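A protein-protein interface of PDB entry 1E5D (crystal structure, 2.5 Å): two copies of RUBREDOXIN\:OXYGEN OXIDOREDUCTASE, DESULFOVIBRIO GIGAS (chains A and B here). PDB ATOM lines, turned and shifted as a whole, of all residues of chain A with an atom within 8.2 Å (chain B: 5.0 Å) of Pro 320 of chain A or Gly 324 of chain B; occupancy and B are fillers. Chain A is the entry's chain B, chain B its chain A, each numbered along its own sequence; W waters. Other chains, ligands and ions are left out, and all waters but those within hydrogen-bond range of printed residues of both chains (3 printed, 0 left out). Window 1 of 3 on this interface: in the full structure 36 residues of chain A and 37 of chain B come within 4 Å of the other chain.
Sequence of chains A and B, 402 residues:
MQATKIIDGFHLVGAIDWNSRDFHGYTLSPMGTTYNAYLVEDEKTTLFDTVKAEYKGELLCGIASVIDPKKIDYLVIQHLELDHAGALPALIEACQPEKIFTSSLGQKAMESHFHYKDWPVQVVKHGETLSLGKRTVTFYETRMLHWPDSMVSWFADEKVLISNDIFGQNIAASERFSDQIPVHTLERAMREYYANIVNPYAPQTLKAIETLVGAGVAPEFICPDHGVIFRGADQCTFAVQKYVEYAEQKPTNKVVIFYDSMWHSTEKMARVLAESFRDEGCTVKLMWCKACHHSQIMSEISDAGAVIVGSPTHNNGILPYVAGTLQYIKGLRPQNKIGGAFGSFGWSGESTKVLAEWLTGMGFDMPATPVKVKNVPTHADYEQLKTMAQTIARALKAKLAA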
ATOM      1  N   ASP A 260      19.344 -26.822  12.630  1.00  0.00           N
ATOM      2  CA  ASP A 260      20.723 -26.583  12.252  1.00  0.00           C
ATOM      3  C   ASP A 260      20.991 -25.087  12.438  1.00  0.00           C
ATOM      4  O   ASP A 260      20.041 -24.326  12.603  1.00  0.00           O
ATOM      5  CB  ASP A 260      21.065 -27.050  10.840  1.00  0.00           C
ATOM      6  CG  ASP A 260      22.568 -27.254  10.688  1.00  0.00           C
ATOM      7  OD1 ASP A 260      23.302 -26.937  11.651  1.00  0.00           O
ATOM      8  OD2 ASP A 260      23.012 -27.725   9.621  1.00  0.00           O
ATOM      9  N   MET A 262      24.211 -21.730  11.899  1.00  0.00           N
ATOM     10  CA  MET A 262      25.553 -21.309  11.515  1.00  0.00           C
ATOM     11  C   MET A 262      26.235 -20.568  12.659  1.00  0.00           C
ATOM     12  O   MET A 262      27.396 -20.852  12.952  1.00  0.00           O
ATOM     13  CB  MET A 262      25.464 -20.429  10.265  1.00  0.00           C
ATOM     14  CG  MET A 262      24.597 -21.047   9.176  1.00  0.00           C
ATOM     15  SD  MET A 262      24.258 -19.940   7.803  1.00  0.00           S
ATOM     16  CE  MET A 262      22.750 -19.151   8.333  1.00  0.00           C
ATOM     17  N   CYS A 289      21.203 -31.442  13.492  1.00  0.00           N
ATOM     18  CA  CYS A 289      21.329 -32.130  12.211  1.00  0.00           C
ATOM     19  C   CYS A 289      22.766 -32.456  11.858  1.00  0.00           C
ATOM     20  O   CYS A 289      23.007 -33.420  11.133  1.00  0.00           O
ATOM     21  CB  CYS A 289      20.707 -31.295  11.089  1.00  0.00           C
ATOM     22  SG  CYS A 289      18.906 -31.292  11.196  1.00  0.00           S
ATOM     23  N   LYS A 290      23.750 -31.705  12.344  1.00  0.00           N
ATOM     24  CA  LYS A 290      25.118 -32.068  11.947  1.00  0.00           C
ATOM     25  C   LYS A 290      25.658 -33.221  12.781  1.00  0.00           C
ATOM     26  O   LYS A 290      26.676 -33.820  12.426  1.00  0.00           O
ATOM     27  CB  LYS A 290      26.016 -30.829  12.024  1.00  0.00           C
ATOM     28  CG  LYS A 290      26.166 -30.165  10.656  1.00  0.00           C
ATOM     29  CD  LYS A 290      26.897 -28.839  10.771  1.00  0.00           C
ATOM     30  CE  LYS A 290      26.640 -27.942   9.565  1.00  0.00           C
ATOM     31  NZ  LYS A 290      25.945 -26.698   9.996  1.00  0.00           N
ATOM     32  N   SER A 311      15.555 -23.653  11.858  1.00  0.00           N
ATOM     33  CA  SER A 311      16.596 -23.288  10.918  1.00  0.00           C
ATOM     34  C   SER A 311      16.723 -21.773  10.837  1.00  0.00           C
ATOM     35  O   SER A 311      15.749 -21.027  10.879  1.00  0.00           O
ATOM     36  CB  SER A 311      16.326 -23.870   9.536  1.00  0.00           C
ATOM     37  OG  SER A 311      17.368 -23.470   8.653  1.00  0.00           O
ATOM     38  N   PRO A 312      17.951 -21.290  10.720  1.00  0.00           N
ATOM     39  CA  PRO A 312      18.134 -19.868  10.407  1.00  0.00           C
ATOM     40  C   PRO A 312      17.718 -19.643   8.961  1.00  0.00           C
ATOM     41  O   PRO A 312      17.566 -20.609   8.195  1.00  0.00           O
ATOM     42  CB  PRO A 312      19.640 -19.678  10.550  1.00  0.00           C
ATOM     43  CG  PRO A 312      20.209 -21.036  10.263  1.00  0.00           C
ATOM     44  CD  PRO A 312      19.227 -22.014  10.856  1.00  0.00           C
ATOM     45  N   HIS A 314      18.824 -19.113   5.430  1.00  0.00           N
ATOM     46  CA  HIS A 314      20.065 -19.178   4.668  1.00  0.00           C
ATOM     47  C   HIS A 314      19.748 -19.024   3.184  1.00  0.00           C
ATOM     48  O   HIS A 314      19.097 -19.930   2.655  1.00  0.00           O
ATOM     49  CB  HIS A 314      20.774 -20.507   4.915  1.00  0.00           C
ATOM     50  CG  HIS A 314      22.065 -20.679   4.180  1.00  0.00           C
ATOM     51  ND1 HIS A 314      22.243 -21.653   3.222  1.00  0.00           N
ATOM     52  CD2 HIS A 314      23.236 -20.002   4.261  1.00  0.00           C
ATOM     53  CE1 HIS A 314      23.475 -21.574   2.746  1.00  0.00           C
ATOM     54  NE2 HIS A 314      24.097 -20.576   3.360  1.00  0.00           N
ATOM     55  N   ASN A 315      20.191 -17.935   2.571  1.00  0.00           N
ATOM     56  CA  ASN A 315      19.905 -17.707   1.157  1.00  0.00           C
ATOM     57  C   ASN A 315      18.421 -17.917   0.841  1.00  0.00           C
ATOM     58  O   ASN A 315      18.079 -18.709  -0.041  1.00  0.00           O
ATOM     59  CB  ASN A 315      20.762 -18.615   0.270  1.00  0.00           C
ATOM     60  CG  ASN A 315      22.253 -18.424   0.470  1.00  0.00           C
ATOM     61  OD1 ASN A 315      23.055 -19.349   0.286  1.00  0.00           O
ATOM     62  ND2 ASN A 315      22.653 -17.219   0.856  1.00  0.00           N
ATOM     63  N   GLY A 317      16.009 -19.404   2.255  1.00  0.00           N
ATOM     64  CA  GLY A 317      15.447 -20.706   2.584  1.00  0.00           C
ATOM     65  C   GLY A 317      16.049 -21.201   3.893  1.00  0.00           C
ATOM     66  O   GLY A 317      16.528 -20.418   4.717  1.00  0.00           O
ATOM     67  N   ILE A 318      16.029 -22.501   4.084  1.00  0.00           N
ATOM     68  CA  ILE A 318      16.537 -23.200   5.243  1.00  0.00           C
ATOM     69  C   ILE A 318      17.841 -23.914   4.917  1.00  0.00           C
ATOM     70  O   ILE A 318      18.176 -24.125   3.750  1.00  0.00           O
ATOM     71  CB  ILE A 318      15.502 -24.231   5.727  1.00  0.00           C
ATOM     72  CG1 ILE A 318      15.273 -25.368   4.725  1.00  0.00           C
ATOM     73  CG2 ILE A 318      14.203 -23.528   6.088  1.00  0.00           C
ATOM     74  CD1 ILE A 318      14.431 -26.499   5.273  1.00  0.00           C
ATOM     75  N   LEU A 319      18.573 -24.280   5.966  1.00  0.00           N
ATOM     76  CA  LEU A 319      19.858 -24.962   5.781  1.00  0.00           C
ATOM     77  C   LEU A 319      19.674 -26.314   5.099  1.00  0.00           C
ATOM     78  O   LEU A 319      18.692 -27.035   5.281  1.00  0.00           O
ATOM     79  CB  LEU A 319      20.560 -25.116   7.135  1.00  0.00           C
ATOM     80  CG  LEU A 319      21.035 -23.819   7.792  1.00  0.00           C
ATOM     81  CD1 LEU A 319      21.485 -24.047   9.222  1.00  0.00           C
ATOM     82  CD2 LEU A 319      22.153 -23.203   6.964  1.00  0.00           C
ATOM     83  N   PRO A 320      20.653 -26.690   4.290  1.00  0.00           N
ATOM     84  CA  PRO A 320      20.593 -27.904   3.486  1.00  0.00           C
ATOM     85  C   PRO A 320      20.241 -29.149   4.295  1.00  0.00           C
ATOM     86  O   PRO A 320      19.465 -29.991   3.836  1.00  0.00           O
ATOM     87  CB  PRO A 320      22.037 -28.052   2.991  1.00  0.00           C
ATOM     88  CG  PRO A 320      22.574 -26.664   2.974  1.00  0.00           C
ATOM     89  CD  PRO A 320      21.917 -25.952   4.123  1.00  0.00           C
ATOM     90  N   TYR A 321      20.846 -29.247   5.483  1.00  0.00           N
ATOM     91  CA  TYR A 321      20.711 -30.463   6.283  1.00  0.00           C
ATOM     92  C   TYR A 321      19.325 -30.548   6.904  1.00  0.00           C
ATOM     93  O   TYR A 321      18.822 -31.644   7.130  1.00  0.00           O
ATOM     94  CB  TYR A 321      21.787 -30.545   7.368  1.00  0.00           C
ATOM     95  CG  TYR A 321      23.149 -30.914   6.820  1.00  0.00           C
ATOM     96  CD1 TYR A 321      23.250 -31.688   5.666  1.00  0.00           C
ATOM     97  CD2 TYR A 321      24.315 -30.489   7.452  1.00  0.00           C
ATOM     98  CE1 TYR A 321      24.488 -32.034   5.155  1.00  0.00           C
ATOM     99  CE2 TYR A 321      25.553 -30.831   6.939  1.00  0.00           C
ATOM    100  CZ  TYR A 321      25.630 -31.599   5.798  1.00  0.00           C
ATOM    101  OH  TYR A 321      26.857 -31.942   5.289  1.00  0.00           O
ATOM    102  N   VAL A 322      18.725 -29.388   7.170  1.00  0.00           N
ATOM    103  CA  VAL A 322      17.350 -29.411   7.663  1.00  0.00           C
ATOM    104  C   VAL A 322      16.402 -29.775   6.530  1.00  0.00           C
ATOM    105  O   VAL A 322      15.452 -30.540   6.665  1.00  0.00           O
ATOM    106  CB  VAL A 322      16.940 -28.063   8.277  1.00  0.00           C
ATOM    107  CG1 VAL A 322      15.519 -28.153   8.817  1.00  0.00           C
ATOM    108  CG2 VAL A 322      17.903 -27.657   9.380  1.00  0.00           C
ATOM    109  N   ALA A 323      16.661 -29.212   5.350  1.00  0.00           N
ATOM    110  CA  ALA A 323      15.839 -29.548   4.187  1.00  0.00           C
ATOM    111  C   ALA A 323      15.922 -31.040   3.890  1.00  0.00           C
ATOM    112  O   ALA A 323      14.908 -31.719   3.767  1.00  0.00           O
ATOM    113  CB  ALA A 323      16.258 -28.719   2.988  1.00  0.00           C
ATOM    114  N   GLY A 324      17.127 -31.587   3.785  1.00  0.00           N
ATOM    115  CA  GLY A 324      17.275 -33.015   3.543  1.00  0.00           C
ATOM    116  C   GLY A 324      16.528 -33.856   4.555  1.00  0.00           C
ATOM    117  O   GLY A 324      15.778 -34.771   4.216  1.00  0.00           O
ATOM    118  N   THR A 325      16.699 -33.563   5.841  1.00  0.00           N
ATOM    119  CA  THR A 325      16.012 -34.319   6.876  1.00  0.00           C
ATOM    120  C   THR A 325      14.502 -34.204   6.746  1.00  0.00           C
ATOM    121  O   THR A 325      13.771 -35.159   6.973  1.00  0.00           O
ATOM    122  CB  THR A 325      16.414 -33.816   8.276  1.00  0.00           C
ATOM    123  OG1 THR A 325      17.834 -33.933   8.409  1.00  0.00           O
ATOM    124  CG2 THR A 325      15.759 -34.677   9.347  1.00  0.00           C
ATOM    125  N   LEU A 326      14.042 -33.003   6.384  1.00  0.00           N
ATOM    126  CA  LEU A 326      12.601 -32.820   6.237  1.00  0.00           C
ATOM    127  C   LEU A 326      12.082 -33.690   5.093  1.00  0.00           C
ATOM    128  O   LEU A 326      11.012 -34.284   5.213  1.00  0.00           O
ATOM    129  CB  LEU A 326      12.242 -31.354   6.013  1.00  0.00           C
ATOM    130  CG  LEU A 326      12.288 -30.481   7.272  1.00  0.00           C
ATOM    131  CD1 LEU A 326      12.041 -29.013   6.949  1.00  0.00           C
ATOM    132  CD2 LEU A 326      11.282 -30.978   8.300  1.00  0.00           C
ATOM    133  N   GLN A 327      12.847 -33.751   4.003  1.00  0.00           N
ATOM    134  CA  GLN A 327      12.413 -34.495   2.830  1.00  0.00           C
ATOM    135  C   GLN A 327      12.272 -35.969   3.192  1.00  0.00           C
ATOM    136  O   GLN A 327      11.372 -36.665   2.734  1.00  0.00           O
ATOM    137  CB  GLN A 327      13.397 -34.353   1.672  1.00  0.00           C
ATOM    138  CG  GLN A 327      12.981 -35.106   0.411  1.00  0.00           C
ATOM    139  CD  GLN A 327      11.591 -34.693  -0.037  1.00  0.00           C
ATOM    140  OE1 GLN A 327      11.357 -33.514  -0.307  1.00  0.00           O
ATOM    141  NE2 GLN A 327      10.673 -35.651  -0.104  1.00  0.00           N
ATOM    142  N   HIS B 294      27.924 -30.588  -0.149  1.00  0.00           N
ATOM    143  CA  HIS B 294      27.168 -29.706  -1.047  1.00  0.00           C
ATOM    144  C   HIS B 294      28.022 -28.518  -1.479  1.00  0.00           C
ATOM    145  O   HIS B 294      27.922 -28.015  -2.597  1.00  0.00           O
ATOM    146  CB  HIS B 294      25.875 -29.222  -0.410  1.00  0.00           C
ATOM    147  CG  HIS B 294      25.916 -28.668   0.969  1.00  0.00           C
ATOM    148  ND1 HIS B 294      25.553 -29.422   2.068  1.00  0.00           N
ATOM    149  CD2 HIS B 294      26.246 -27.448   1.452  1.00  0.00           C
ATOM    150  CE1 HIS B 294      25.671 -28.688   3.164  1.00  0.00           C
ATOM    151  NE2 HIS B 294      26.093 -27.484   2.819  1.00  0.00           N
ATOM    152  N   PRO B 320      17.357 -37.785   0.304  1.00  0.00           N
ATOM    153  CA  PRO B 320      17.539 -36.633   1.182  1.00  0.00           C
ATOM    154  C   PRO B 320      18.745 -35.782   0.808  1.00  0.00           C
ATOM    155  O   PRO B 320      18.661 -34.559   0.734  1.00  0.00           O
ATOM    156  CB  PRO B 320      17.811 -37.296   2.535  1.00  0.00           C
ATOM    157  CG  PRO B 320      17.123 -38.617   2.454  1.00  0.00           C
ATOM    158  CD  PRO B 320      17.237 -39.065   1.034  1.00  0.00           C
ATOM    159  N   TYR B 321      19.877 -36.433   0.582  1.00  0.00           N
ATOM    160  CA  TYR B 321      21.124 -35.745   0.292  1.00  0.00           C
ATOM    161  C   TYR B 321      21.063 -35.044  -1.057  1.00  0.00           C
ATOM    162  O   TYR B 321      21.711 -34.018  -1.280  1.00  0.00           O
ATOM    163  CB  TYR B 321      22.285 -36.739   0.316  1.00  0.00           C
ATOM    164  CG  TYR B 321      22.652 -37.201   1.700  1.00  0.00           C
ATOM    165  CD1 TYR B 321      22.383 -36.392   2.796  1.00  0.00           C
ATOM    166  CD2 TYR B 321      23.255 -38.431   1.913  1.00  0.00           C
ATOM    167  CE1 TYR B 321      22.710 -36.794   4.077  1.00  0.00           C
ATOM    168  CE2 TYR B 321      23.587 -38.842   3.196  1.00  0.00           C
ATOM    169  CZ  TYR B 321      23.310 -38.025   4.268  1.00  0.00           C
ATOM    170  OH  TYR B 321      23.638 -38.422   5.543  1.00  0.00           O
ATOM    171  N   VAL B 322      20.266 -35.604  -1.971  1.00  0.00           N
ATOM    172  CA  VAL B 322      20.075 -34.892  -3.235  1.00  0.00           C
ATOM    173  C   VAL B 322      19.228 -33.644  -3.007  1.00  0.00           C
ATOM    174  O   VAL B 322      19.516 -32.561  -3.503  1.00  0.00           O
ATOM    175  CB  VAL B 322      19.433 -35.796  -4.300  1.00  0.00           C
ATOM    176  CG1 VAL B 322      19.188 -34.995  -5.566  1.00  0.00           C
ATOM    177  CG2 VAL B 322      20.334 -36.986  -4.582  1.00  0.00           C
ATOM    178  N   ALA B 323      18.170 -33.802  -2.228  1.00  0.00           N
ATOM    179  CA  ALA B 323      17.325 -32.671  -1.870  1.00  0.00           C
ATOM    180  C   ALA B 323      18.113 -31.588  -1.151  1.00  0.00           C
ATOM    181  O   ALA B 323      17.992 -30.402  -1.476  1.00  0.00           O
ATOM    182  CB  ALA B 323      16.164 -33.129  -0.994  1.00  0.00           C
ATOM    183  N   GLY B 324      18.925 -31.970  -0.167  1.00  0.00           N
ATOM    184  CA  GLY B 324      19.690 -30.973   0.578  1.00  0.00           C
ATOM    185  C   GLY B 324      20.649 -30.200  -0.307  1.00  0.00           C
ATOM    186  O   GLY B 324      20.830 -28.990  -0.160  1.00  0.00           O
ATOM    187  N   THR B 325      21.284 -30.902  -1.241  1.00  0.00           N
ATOM    188  CA  THR B 325      22.222 -30.266  -2.160  1.00  0.00           C
ATOM    189  C   THR B 325      21.531 -29.331  -3.130  1.00  0.00           C
ATOM    190  O   THR B 325      22.017 -28.247  -3.458  1.00  0.00           O
ATOM    191  CB  THR B 325      22.977 -31.353  -2.951  1.00  0.00           C
ATOM    192  OG1 THR B 325      23.671 -32.155  -1.977  1.00  0.00           O
ATOM    193  CG2 THR B 325      24.001 -30.753  -3.895  1.00  0.00           C
ATOM    194  N   LEU B 326      20.365 -29.754  -3.617  1.00  0.00           N
ATOM    195  CA  LEU B 326      19.623 -28.862  -4.512  1.00  0.00           C
ATOM    196  C   LEU B 326      19.169 -27.628  -3.744  1.00  0.00           C
ATOM    197  O   LEU B 326      19.249 -26.512  -4.264  1.00  0.00           O
ATOM    198  CB  LEU B 326      18.442 -29.587  -5.148  1.00  0.00           C
ATOM    199  CG  LEU B 326      18.838 -30.554  -6.268  1.00  0.00           C
ATOM    200  CD1 LEU B 326      17.688 -31.494  -6.582  1.00  0.00           C
ATOM    201  CD2 LEU B 326      19.275 -29.769  -7.490  1.00  0.00           C
ATOM    202  N   GLN B 327      18.717 -27.818  -2.509  1.00  0.00           N
ATOM    203  CA  GLN B 327      18.334 -26.669  -1.692  1.00  0.00           C
ATOM    204  C   GLN B 327      19.502 -25.685  -1.602  1.00  0.00           C
ATOM    205  O   GLN B 327      19.355 -24.496  -1.843  1.00  0.00           O
ATOM    206  CB  GLN B 327      17.903 -27.053  -0.276  1.00  0.00           C
ATOM    207  CG  GLN B 327      17.389 -25.870   0.547  1.00  0.00           C
ATOM    208  CD  GLN B 327      16.209 -25.207  -0.152  1.00  0.00           C
ATOM    209  OE1 GLN B 327      15.151 -25.829  -0.273  1.00  0.00           O
ATOM    210  NE2 GLN B 327      16.393 -23.974  -0.620  1.00  0.00           N
ATOM    211  N   TYR B 328      20.670 -26.221  -1.254  1.00  0.00           N
ATOM    212  CA  TYR B 328      21.859 -25.386  -1.128  1.00  0.00           C
ATOM    213  C   TYR B 328      22.088 -24.628  -2.428  1.00  0.00           C
ATOM    214  O   TYR B 328      22.286 -23.422  -2.442  1.00  0.00           O
ATOM    215  CB  TYR B 328      23.080 -26.234  -0.817  1.00  0.00           C
ATOM    216  CG  TYR B 328      24.344 -25.462  -0.548  1.00  0.00           C
ATOM    217  CD1 TYR B 328      24.494 -24.771   0.646  1.00  0.00           C
ATOM    218  CD2 TYR B 328      25.394 -25.423  -1.459  1.00  0.00           C
ATOM    219  CE1 TYR B 328      25.643 -24.062   0.919  1.00  0.00           C
ATOM    220  CE2 TYR B 328      26.552 -24.709  -1.187  1.00  0.00           C
ATOM    221  CZ  TYR B 328      26.673 -24.027   0.004  1.00  0.00           C
ATOM    222  OH  TYR B 328      27.809 -23.312   0.297  1.00  0.00           O
HETATM  223  O   HOH W   1      21.818 -21.669  -0.222  1.00  0.00           O
HETATM  224  O   HOH W   2      26.383 -32.510   2.272  1.00  0.00           O
HETATM  225  O   HOH W   3      13.956 -23.802   1.828  1.00  0.00           O
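A ring nitrogen (NE2) of His 314 of chain A sits close to the side-chain amide oxygen (OD1) of Asn 315 of chain A (3.5 Å).
The side-chain hydroxyl of Thr 325 of chain A lies within hydrogen-bond range of the backbone carbonyl oxygen of Tyr 321 of chain A (2.8 Å).
His 314 of chain A touches Tyr 328 of chain B.
Ile 318 of chain A touches Gln 327 of chain B (O to CG, 3.7 Å).
NE2 of His 294 of chain B touches CG of Pro 320 of chain A (3.6 Å).
Gly 324 of chain B touches Pro 320 of chain A (CA to O, 3.4 Å).
CG of Pro 320 of chain A touches CD1 of Tyr 328 of chain B, at 3.6 Å.
His 294 of chain B touches Tyr 321 of chain A (CE1 to CZ, 3.9 Å).
CG of Gln 327 of chain B touches CB of Ala 323 of chain A, at 3.9 Å.
O of Pro 320 of chain B touches CA of Gly 324 of chain A (3.5 Å).
Of the printed residues of chain B, Ile 318 of chain A touches Gln 327.
Of the printed residues of chain B, Tyr 321 of chain A touches His 294.
Printed residues of chain B within 4 Å of Gly 324 of chain A: Pro 320 (3.5 Å).
Leu 326 of chain A touches none of the printed residues of chain B.
Printed residues of chain A within 4 Å of His 294 of chain B: Pro 320 and Tyr 321.
Printed residues of chain A within 4 Å of Pro 320 of chain B: Gly 324 (3.5 Å).
Val 322 of chain B touches none of the printed residues of chain A.
Of chain A, only Pro 320 comes within 4 Å of Gly 324 of chain B.
The nearest residue of chain B that does not touch Pro 320 of chain A is Gln 327 of chain B (4.7 Å).
Of the 10 printed residues of chain B, 5 touch a printed residue of chain A.
Hydrophobic or aromatic side chains of chain B within 4 Å of the printed part of chain A: His 294, Pro 320 and Tyr 328.
Of the 19 printed residues of chain A, 6 touch a printed residue of chain B.
Along chain A the printed residues that touch a printed residue of chain B span positions 314 to 324.
Among the printed residues, 8 pairs touch across the chains.
Pro 320 of chain A touches Gly 324 of chain B, and with the chains exchanged Gly 324 of chain A touches Pro 320 of chain B.
Ala 323 of chain A touches Gln 327 of chain B, but with the chains exchanged Gln 327 of chain A does not touch Ala 323 of chain B (4.002 Å).
Positions printed for both chains: 320, 321, 322, 323, 324, 325, 326 and 327.
Water W1 lies within hydrogen-bond range of OD1 of Asn 315 of chain A, O of Tyr 328 of chain B and ND1 of His 314 of chain A.
Water W2 lies within hydrogen-bond range of OH of Tyr 321 of chain A and ND1 of His 294 of chain B.
Water W3 bridges OE1 of Gln 327 of chain B (3.2 Å) and N of Ile 318 of chain A (3.3 Å).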
